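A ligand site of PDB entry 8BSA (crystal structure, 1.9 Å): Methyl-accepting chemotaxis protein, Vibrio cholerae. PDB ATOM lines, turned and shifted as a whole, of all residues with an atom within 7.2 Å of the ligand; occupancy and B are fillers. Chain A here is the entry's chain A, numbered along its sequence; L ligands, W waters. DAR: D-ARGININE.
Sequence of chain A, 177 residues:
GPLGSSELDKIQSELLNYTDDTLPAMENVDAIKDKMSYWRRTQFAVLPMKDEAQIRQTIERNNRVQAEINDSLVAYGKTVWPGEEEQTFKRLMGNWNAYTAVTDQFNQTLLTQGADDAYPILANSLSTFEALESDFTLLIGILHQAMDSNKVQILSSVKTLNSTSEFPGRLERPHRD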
ATOM      1  N   GLU A  14      -1.657  25.994  26.972  1.00  0.00           N
ATOM      2  CA  GLU A  14      -2.807  26.084  26.090  1.00  0.00           C
ATOM      3  C   GLU A  14      -2.951  27.496  25.544  1.00  0.00           C
ATOM      4  O   GLU A  14      -3.217  27.679  24.344  1.00  0.00           O
ATOM      5  CB  GLU A  14      -4.084  25.676  26.823  1.00  0.00           C
ATOM      6  CG  GLU A  14      -4.310  24.163  26.951  1.00  0.00           C
ATOM      7  CD  GLU A  14      -4.048  23.374  25.666  1.00  0.00           C
ATOM      8  OE1 GLU A  14      -4.421  23.837  24.567  1.00  0.00           O
ATOM      9  OE2 GLU A  14      -3.471  22.264  25.765  1.00  0.00           O
ATOM     10  N   ASN A  17      -0.062  28.139  22.939  1.00  0.00           N
ATOM     11  CA  ASN A  17      -0.353  27.475  21.683  1.00  0.00           C
ATOM     12  C   ASN A  17      -1.430  28.220  20.897  1.00  0.00           C
ATOM     13  O   ASN A  17      -1.361  28.302  19.667  1.00  0.00           O
ATOM     14  CB  ASN A  17      -0.783  26.039  21.973  1.00  0.00           C
ATOM     15  CG  ASN A  17      -1.430  25.376  20.794  1.00  0.00           C
ATOM     16  OD1 ASN A  17      -0.739  24.953  19.866  1.00  0.00           O
ATOM     17  ND2 ASN A  17      -2.748  25.298  20.802  1.00  0.00           N
ATOM     18  N   TYR A  18      -2.405  28.794  21.601  1.00  0.00           N
ATOM     19  CA  TYR A  18      -3.501  29.506  20.938  1.00  0.00           C
ATOM     20  C   TYR A  18      -3.027  30.828  20.362  1.00  0.00           C
ATOM     21  O   TYR A  18      -3.313  31.165  19.210  1.00  0.00           O
ATOM     22  CB  TYR A  18      -4.634  29.729  21.950  1.00  0.00           C
ATOM     23  CG  TYR A  18      -5.791  30.511  21.400  1.00  0.00           C
ATOM     24  CD1 TYR A  18      -6.503  30.027  20.314  1.00  0.00           C
ATOM     25  CD2 TYR A  18      -6.166  31.731  21.957  1.00  0.00           C
ATOM     26  CE1 TYR A  18      -7.568  30.734  19.791  1.00  0.00           C
ATOM     27  CE2 TYR A  18      -7.233  32.447  21.424  1.00  0.00           C
ATOM     28  CZ  TYR A  18      -7.931  31.937  20.339  1.00  0.00           C
ATOM     29  OH  TYR A  18      -8.998  32.624  19.806  1.00  0.00           O
ATOM     30  N   ASP A  20       0.194  31.937  19.951  1.00  0.00           N
ATOM     31  CA  ASP A  20       1.433  31.937  19.181  1.00  0.00           C
ATOM     32  C   ASP A  20       1.499  30.883  18.086  1.00  0.00           C
ATOM     33  O   ASP A  20       2.442  30.895  17.288  1.00  0.00           O
ATOM     34  CB  ASP A  20       2.653  31.741  20.084  1.00  0.00           C
ATOM     35  CG  ASP A  20       2.903  32.897  21.052  1.00  0.00           C
ATOM     36  OD1 ASP A  20       2.159  33.904  21.027  1.00  0.00           O
ATOM     37  OD2 ASP A  20       3.905  32.813  21.800  1.00  0.00           O
ATOM     38  N   ASP A  21       0.571  29.927  18.061  1.00  0.00           N
ATOM     39  CA  ASP A  21       0.521  28.981  16.957  1.00  0.00           C
ATOM     40  C   ASP A  21      -0.805  29.046  16.229  1.00  0.00           C
ATOM     41  O   ASP A  21      -0.829  29.314  15.022  1.00  0.00           O
ATOM     42  CB  ASP A  21       0.785  27.544  17.423  1.00  0.00           C
ATOM     43  CG  ASP A  21       1.034  26.590  16.247  1.00  0.00           C
ATOM     44  OD1 ASP A  21       2.160  26.589  15.682  1.00  0.00           O
ATOM     45  OD2 ASP A  21       0.106  25.876  15.857  1.00  0.00           O
ATOM     46  N   THR A  22      -1.915  28.794  16.922  1.00  0.00           N
ATOM     47  CA  THR A  22      -3.192  28.690  16.226  1.00  0.00           C
ATOM     48  C   THR A  22      -3.603  30.014  15.627  1.00  0.00           C
ATOM     49  O   THR A  22      -3.973  30.089  14.442  1.00  0.00           O
ATOM     50  CB  THR A  22      -4.269  28.180  17.168  1.00  0.00           C
ATOM     51  OG1 THR A  22      -3.883  26.908  17.683  1.00  0.00           O
ATOM     52  CG2 THR A  22      -5.589  28.081  16.427  1.00  0.00           C
ATOM     53  N   LEU A  23      -3.625  31.067  16.428  1.00  0.00           N
ATOM     54  CA  LEU A  23      -4.087  32.351  15.921  1.00  0.00           C
ATOM     55  C   LEU A  23      -3.217  32.824  14.772  1.00  0.00           C
ATOM     56  O   LEU A  23      -3.766  33.247  13.742  1.00  0.00           O
ATOM     57  CB  LEU A  23      -4.138  33.395  17.044  1.00  0.00           C
ATOM     58  CG  LEU A  23      -5.423  33.398  17.868  1.00  0.00           C
ATOM     59  CD1 LEU A  23      -5.379  34.417  18.986  1.00  0.00           C
ATOM     60  CD2 LEU A  23      -6.628  33.621  16.958  1.00  0.00           C
ATOM     61  N   PRO A  24      -1.895  32.783  14.875  1.00  0.00           N
ATOM     62  CA  PRO A  24      -1.086  33.214  13.718  1.00  0.00           C
ATOM     63  C   PRO A  24      -1.360  32.367  12.497  1.00  0.00           C
ATOM     64  O   PRO A  24      -1.399  32.895  11.393  1.00  0.00           O
ATOM     65  CB  PRO A  24       0.356  33.087  14.216  1.00  0.00           C
ATOM     66  CG  PRO A  24       0.228  33.292  15.708  1.00  0.00           C
ATOM     67  CD  PRO A  24      -1.065  32.572  16.069  1.00  0.00           C
ATOM     68  N   ALA A  25      -1.555  31.061  12.665  1.00  0.00           N
ATOM     69  CA  ALA A  25      -1.942  30.240  11.514  1.00  0.00           C
ATOM     70  C   ALA A  25      -3.210  30.789  10.896  1.00  0.00           C
ATOM     71  O   ALA A  25      -3.283  31.049   9.682  1.00  0.00           O
ATOM     72  CB  ALA A  25      -2.154  28.788  11.924  1.00  0.00           C
ATOM     73  N   MET A  26      -4.244  30.976  11.720  1.00  0.00           N
ATOM     74  CA  MET A  26      -5.532  31.389  11.182  1.00  0.00           C
ATOM     75  C   MET A  26      -5.409  32.755  10.532  1.00  0.00           C
ATOM     76  O   MET A  26      -5.939  32.975   9.445  1.00  0.00           O
ATOM     77  CB  MET A  26      -6.579  31.407  12.284  1.00  0.00           C
ATOM     78  CG  MET A  26      -7.928  31.956  11.825  1.00  0.00           C
ATOM     79  SD  MET A  26      -8.917  30.831  10.822  1.00  0.00           S
ATOM     80  CE  MET A  26      -8.259  31.091   9.179  1.00  0.00           C
ATOM     81  N   VAL A  29      -3.442  32.225   7.156  1.00  0.00           N
ATOM     82  CA  VAL A  29      -4.217  31.614   6.087  1.00  0.00           C
ATOM     83  C   VAL A  29      -5.324  32.551   5.631  1.00  0.00           C
ATOM     84  O   VAL A  29      -5.593  32.691   4.430  1.00  0.00           O
ATOM     85  CB  VAL A  29      -4.768  30.247   6.542  1.00  0.00           C
ATOM     86  CG1 VAL A  29      -5.650  29.684   5.453  1.00  0.00           C
ATOM     87  CG2 VAL A  29      -3.628  29.321   6.859  1.00  0.00           C
ATOM     88  N   TYR A  76       3.867  29.228   5.365  1.00  0.00           N
ATOM     89  CA  TYR A  76       2.817  28.614   6.147  1.00  0.00           C
ATOM     90  C   TYR A  76       2.962  27.100   6.175  1.00  0.00           C
ATOM     91  O   TYR A  76       2.748  26.461   7.210  1.00  0.00           O
ATOM     92  CB  TYR A  76       1.447  29.032   5.622  1.00  0.00           C
ATOM     93  CG  TYR A  76       0.365  28.167   6.167  1.00  0.00           C
ATOM     94  CD1 TYR A  76      -0.184  28.407   7.418  1.00  0.00           C
ATOM     95  CD2 TYR A  76      -0.064  27.086   5.455  1.00  0.00           C
ATOM     96  CE1 TYR A  76      -1.176  27.569   7.922  1.00  0.00           C
ATOM     97  CE2 TYR A  76      -1.032  26.246   5.941  1.00  0.00           C
ATOM     98  CZ  TYR A  76      -1.587  26.485   7.162  1.00  0.00           C
ATOM     99  OH  TYR A  76      -2.567  25.614   7.589  1.00  0.00           O
ATOM    100  N   GLY A  77       3.360  26.488   5.058  1.00  0.00           N
ATOM    101  CA  GLY A  77       3.517  25.047   5.035  1.00  0.00           C
ATOM    102  C   GLY A  77       4.574  24.512   5.997  1.00  0.00           C
ATOM    103  O   GLY A  77       4.564  23.313   6.314  1.00  0.00           O
ATOM    104  N   LYS A  78       5.485  25.366   6.460  1.00  0.00           N
ATOM    105  CA  LYS A  78       6.479  24.930   7.423  1.00  0.00           C
ATOM    106  C   LYS A  78       5.886  24.833   8.821  1.00  0.00           C
ATOM    107  O   LYS A  78       6.446  24.149   9.678  1.00  0.00           O
ATOM    108  CB  LYS A  78       7.672  25.886   7.412  1.00  0.00           C
ATOM    109  CG  LYS A  78       8.396  25.895   6.050  1.00  0.00           C
ATOM    110  CD  LYS A  78       9.563  26.875   5.996  1.00  0.00           C
ATOM    111  CE  LYS A  78      10.244  26.820   4.640  1.00  0.00           C
ATOM    112  NZ  LYS A  78      10.291  28.164   4.015  1.00  0.00           N
ATOM    113  N   THR A  79       4.747  25.482   9.057  1.00  0.00           N
ATOM    114  CA  THR A  79       4.113  25.504  10.360  1.00  0.00           C
ATOM    115  C   THR A  79       2.986  24.496  10.508  1.00  0.00           C
ATOM    116  O   THR A  79       2.467  24.336  11.624  1.00  0.00           O
ATOM    117  CB  THR A  79       3.563  26.910  10.665  1.00  0.00           C
ATOM    118  OG1 THR A  79       2.375  27.153   9.894  1.00  0.00           O
ATOM    119  CG2 THR A  79       4.591  27.989  10.366  1.00  0.00           C
ATOM    120  N   VAL A  80       2.596  23.811   9.425  1.00  0.00           N
ATOM    121  CA  VAL A  80       1.412  22.952   9.501  1.00  0.00           C
ATOM    122  C   VAL A  80       1.676  21.767  10.403  1.00  0.00           C
ATOM    123  O   VAL A  80       2.787  21.225  10.464  1.00  0.00           O
ATOM    124  CB  VAL A  80       0.947  22.474   8.105  1.00  0.00           C
ATOM    125  CG1 VAL A  80       0.691  23.656   7.209  1.00  0.00           C
ATOM    126  CG2 VAL A  80       1.931  21.481   7.515  1.00  0.00           C
ATOM    127  N   TRP A  81       0.647  21.343  11.098  1.00  0.00           N
ATOM    128  CA  TRP A  81       0.717  20.157  11.929  1.00  0.00           C
ATOM    129  C   TRP A  81       0.383  18.931  11.101  1.00  0.00           C
ATOM    130  O   TRP A  81      -0.298  19.019  10.065  1.00  0.00           O
ATOM    131  CB  TRP A  81      -0.244  20.280  13.099  1.00  0.00           C
ATOM    132  CG  TRP A  81       0.247  21.233  14.116  1.00  0.00           C
ATOM    133  CD1 TRP A  81       1.163  22.217  13.928  1.00  0.00           C
ATOM    134  CD2 TRP A  81      -0.157  21.312  15.489  1.00  0.00           C
ATOM    135  NE1 TRP A  81       1.353  22.919  15.091  1.00  0.00           N
ATOM    136  CE2 TRP A  81       0.559  22.384  16.071  1.00  0.00           C
ATOM    137  CE3 TRP A  81      -1.046  20.585  16.285  1.00  0.00           C
ATOM    138  CZ2 TRP A  81       0.406  22.744  17.409  1.00  0.00           C
ATOM    139  CZ3 TRP A  81      -1.191  20.942  17.628  1.00  0.00           C
ATOM    140  CH2 TRP A  81      -0.467  22.020  18.164  1.00  0.00           C
ATOM    141  N   GLU A  85      -4.433  18.893   8.413  1.00  0.00           N
ATOM    142  CA  GLU A  85      -3.914  20.186   7.961  1.00  0.00           C
ATOM    143  C   GLU A  85      -2.774  20.020   6.953  1.00  0.00           C
ATOM    144  O   GLU A  85      -2.775  20.649   5.892  1.00  0.00           O
ATOM    145  CB  GLU A  85      -3.424  21.026   9.139  1.00  0.00           C
ATOM    146  CG  GLU A  85      -3.123  22.476   8.729  1.00  0.00           C
ATOM    147  CD  GLU A  85      -2.370  23.230   9.784  1.00  0.00           C
ATOM    148  OE1 GLU A  85      -2.043  22.620  10.825  1.00  0.00           O
ATOM    149  OE2 GLU A  85      -2.051  24.435   9.580  1.00  0.00           O
ATOM    150  N   ILE A 142     -10.281  23.867   9.307  1.00  0.00           N
ATOM    151  CA  ILE A 142      -9.433  23.182  10.263  1.00  0.00           C
ATOM    152  C   ILE A 142      -8.919  24.152  11.313  1.00  0.00           C
ATOM    153  O   ILE A 142      -8.906  23.845  12.512  1.00  0.00           O
ATOM    154  CB  ILE A 142      -8.261  22.502   9.521  1.00  0.00           C
ATOM    155  CG1 ILE A 142      -8.778  21.336   8.681  1.00  0.00           C
ATOM    156  CG2 ILE A 142      -7.222  22.033  10.513  1.00  0.00           C
ATOM    157  CD1 ILE A 142      -7.764  20.811   7.663  1.00  0.00           C
ATOM    158  N   LEU A 143      -8.472  25.325  10.896  1.00  0.00           N
ATOM    159  CA  LEU A 143      -7.944  26.285  11.862  1.00  0.00           C
ATOM    160  C   LEU A 143      -9.046  26.897  12.702  1.00  0.00           C
ATOM    161  O   LEU A 143      -8.822  27.159  13.893  1.00  0.00           O
ATOM    162  CB  LEU A 143      -7.160  27.371  11.135  1.00  0.00           C
ATOM    163  CG  LEU A 143      -5.926  26.818  10.418  1.00  0.00           C
ATOM    164  CD1 LEU A 143      -5.362  27.864   9.484  1.00  0.00           C
ATOM    165  CD2 LEU A 143      -4.882  26.353  11.422  1.00  0.00           C
ATOM    166  N   GLN A 145     -11.636  25.231  13.636  1.00  0.00           N
ATOM    167  CA  GLN A 145     -11.813  24.156  14.600  1.00  0.00           C
ATOM    168  C   GLN A 145     -10.714  24.176  15.644  1.00  0.00           C
ATOM    169  O   GLN A 145     -10.980  23.983  16.835  1.00  0.00           O
ATOM    170  CB  GLN A 145     -11.830  22.816  13.873  1.00  0.00           C
ATOM    171  CG  GLN A 145     -12.115  21.631  14.780  1.00  0.00           C
ATOM    172  CD  GLN A 145     -13.405  21.804  15.542  1.00  0.00           C
ATOM    173  OE1 GLN A 145     -14.483  21.760  14.946  1.00  0.00           O
ATOM    174  NE2 GLN A 145     -13.309  21.941  16.868  1.00  0.00           N
ATOM    175  N   ALA A 146      -9.473  24.408  15.218  1.00  0.00           N
ATOM    176  CA  ALA A 146      -8.381  24.467  16.181  1.00  0.00           C
ATOM    177  C   ALA A 146      -8.575  25.615  17.165  1.00  0.00           C
ATOM    178  O   ALA A 146      -8.367  25.454  18.369  1.00  0.00           O
ATOM    179  CB  ALA A 146      -7.033  24.599  15.460  1.00  0.00           C
ATOM    180  N   MET A 147      -8.958  26.786  16.661  1.00  0.00           N
ATOM    181  CA  MET A 147      -9.209  27.916  17.547  1.00  0.00           C
ATOM    182  C   MET A 147     -10.262  27.577  18.576  1.00  0.00           C
ATOM    183  O   MET A 147     -10.122  27.908  19.762  1.00  0.00           O
ATOM    184  CB  MET A 147      -9.661  29.149  16.784  1.00  0.00           C
ATOM    185  CG  MET A 147      -8.704  29.634  15.760  1.00  0.00           C
ATOM    186  SD  MET A 147      -9.350  31.002  14.799  1.00  0.00           S
ATOM    187  CE  MET A 147     -10.015  32.117  16.012  1.00  0.00           C
ATOM    188  N   SER A 149     -11.348  24.620  19.573  1.00  0.00           N
ATOM    189  CA  SER A 149     -10.823  23.565  20.429  1.00  0.00           C
ATOM    190  C   SER A 149      -9.808  24.140  21.421  1.00  0.00           C
ATOM    191  O   SER A 149      -9.798  23.762  22.601  1.00  0.00           O
ATOM    192  CB  SER A 149     -10.186  22.465  19.572  1.00  0.00           C
ATOM    193  OG  SER A 149      -9.735  21.373  20.345  1.00  0.00           O
ATOM    194  N   ASN A 150      -8.959  25.069  20.958  1.00  0.00           N
ATOM    195  CA  ASN A 150      -8.017  25.719  21.859  1.00  0.00           C
ATOM    196  C   ASN A 150      -8.753  26.445  22.979  1.00  0.00           C
ATOM    197  O   ASN A 150      -8.413  26.319  24.160  1.00  0.00           O
ATOM    198  CB  ASN A 150      -7.163  26.739  21.102  1.00  0.00           C
ATOM    199  CG  ASN A 150      -6.096  26.096  20.238  1.00  0.00           C
ATOM    200  OD1 ASN A 150      -5.302  26.787  19.618  1.00  0.00           O
ATOM    201  ND2 ASN A 150      -6.064  24.770  20.225  1.00  0.00           N
HETATM  202  N   DAR L   1      -1.965  25.017  17.127  1.00  0.00           N
HETATM  203  CA  DAR L   1      -2.758  24.008  16.452  1.00  0.00           C
HETATM  204  CB  DAR L   1      -3.481  24.620  15.264  1.00  0.00           C
HETATM  205  CG  DAR L   1      -2.526  25.289  14.334  1.00  0.00           C
HETATM  206  CD  DAR L   1      -1.540  24.282  13.771  1.00  0.00           C
HETATM  207  NE  DAR L   1      -1.168  24.682  12.431  1.00  0.00           N
HETATM  208  CZ  DAR L   1      -0.313  25.662  12.160  1.00  0.00           C
HETATM  209  NH1 DAR L   1       0.369  26.261  13.115  1.00  0.00           N
HETATM  210  NH2 DAR L   1      -0.162  26.056  10.901  1.00  0.00           N
HETATM  211  C   DAR L   1      -3.763  23.388  17.392  1.00  0.00           C
HETATM  212  O   DAR L   1      -4.483  22.494  16.979  1.00  0.00           O
HETATM  213  OXT DAR L   1      -3.871  23.775  18.565  1.00  0.00           O
HETATM  214  O   HOH W   1      -6.617  21.562  18.300  1.00  0.00           O
HETATM  215  O   HOH W   2      -5.052  21.331  14.682  1.00  0.00           O
HETATM  216  O   HOH W   3      -3.550  21.830  20.667  1.00  0.00           O
HETATM  217  O   HOH W   4       1.252  29.140  13.208  1.00  0.00           O
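N of the ligand is in salt-bridge range of OD2 of Asp 21 (2.6 Å). A nitrogen (N) of the ligand lies within hydrogen-bond range of the side-chain hydroxyl (OG1) of Thr 22 (2.8 Å). OE1 of Glu 85 lies within salt-bridge range of NE of the ligand (2.8 Å). The side-chain amide nitrogen of Asn 150 sits at hydrogen-bond distance from an oxygen (OXT) of the ligand, 2.9 Å away. The side-chain amide nitrogen (ND2) of Asn 17 sits at hydrogen-bond distance from an oxygen (OXT) of the ligand (2.9 Å). The backbone carbonyl oxygen of Thr 79 sits close to a nitrogen (NH1) of the ligand, 3.2 Å away. A nitrogen (NH2) of the ligand is in hydrogen-bond range of the side-chain hydroxyl of Thr 79.
The indole nitrogen (NE1) of Trp 81 sits at hydrogen-bond distance from the side-chain carboxylate (OD2) of Asp 21, 3.3 Å away. OD1 of Asn 150 lies within hydrogen-bond range of OG1 of Thr 22 (2.4 Å). O of Asn 17 is in hydrogen-bond range of N of Thr 22, 2.8 Å away. The side-chain carboxylate (OE1) of Glu 85 is in hydrogen-bond range of the backbone NH (N) of Trp 81 (3.0 Å). The side-chain amide oxygen (OD1) of Asn 150 is in hydrogen-bond range of the side-chain amide nitrogen (ND2) of Asn 17 (3.2 Å). ND2 of Asn 150 lies close to O of Ala 146. O of Tyr 76 is in hydrogen-bond range of OG1 of Thr 79.
CB of Ala 25 touches NH2 of the ligand (3.5 Å). Tyr 76 touches the ligand. CA of Val 80 touches NH2 of the ligand (3.8 Å). Trp 81 touches the ligand (CZ2 to N, 3.3 Å). Leu 143 touches the ligand (CD2 to CG, 3.9 Å). Ala 146 touches the ligand (CB to CB, 3.6 Å). Hydrophobic or aromatic side chains within 4 Å of the ligand: Ala 25, Tyr 76, Trp 81, Leu 143 and Ala 146. The nearest printed residue that does not touch the ligand is Tyr 18 (5.9 Å).
Water W4 lies within hydrogen-bond range of the backbone carbonyl oxygen (O) of Asp 21 (2.8 Å), a nitrogen (NH1) of the ligand (3.0 Å) and the backbone NH (N) of Ala 25 (3.4 Å).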
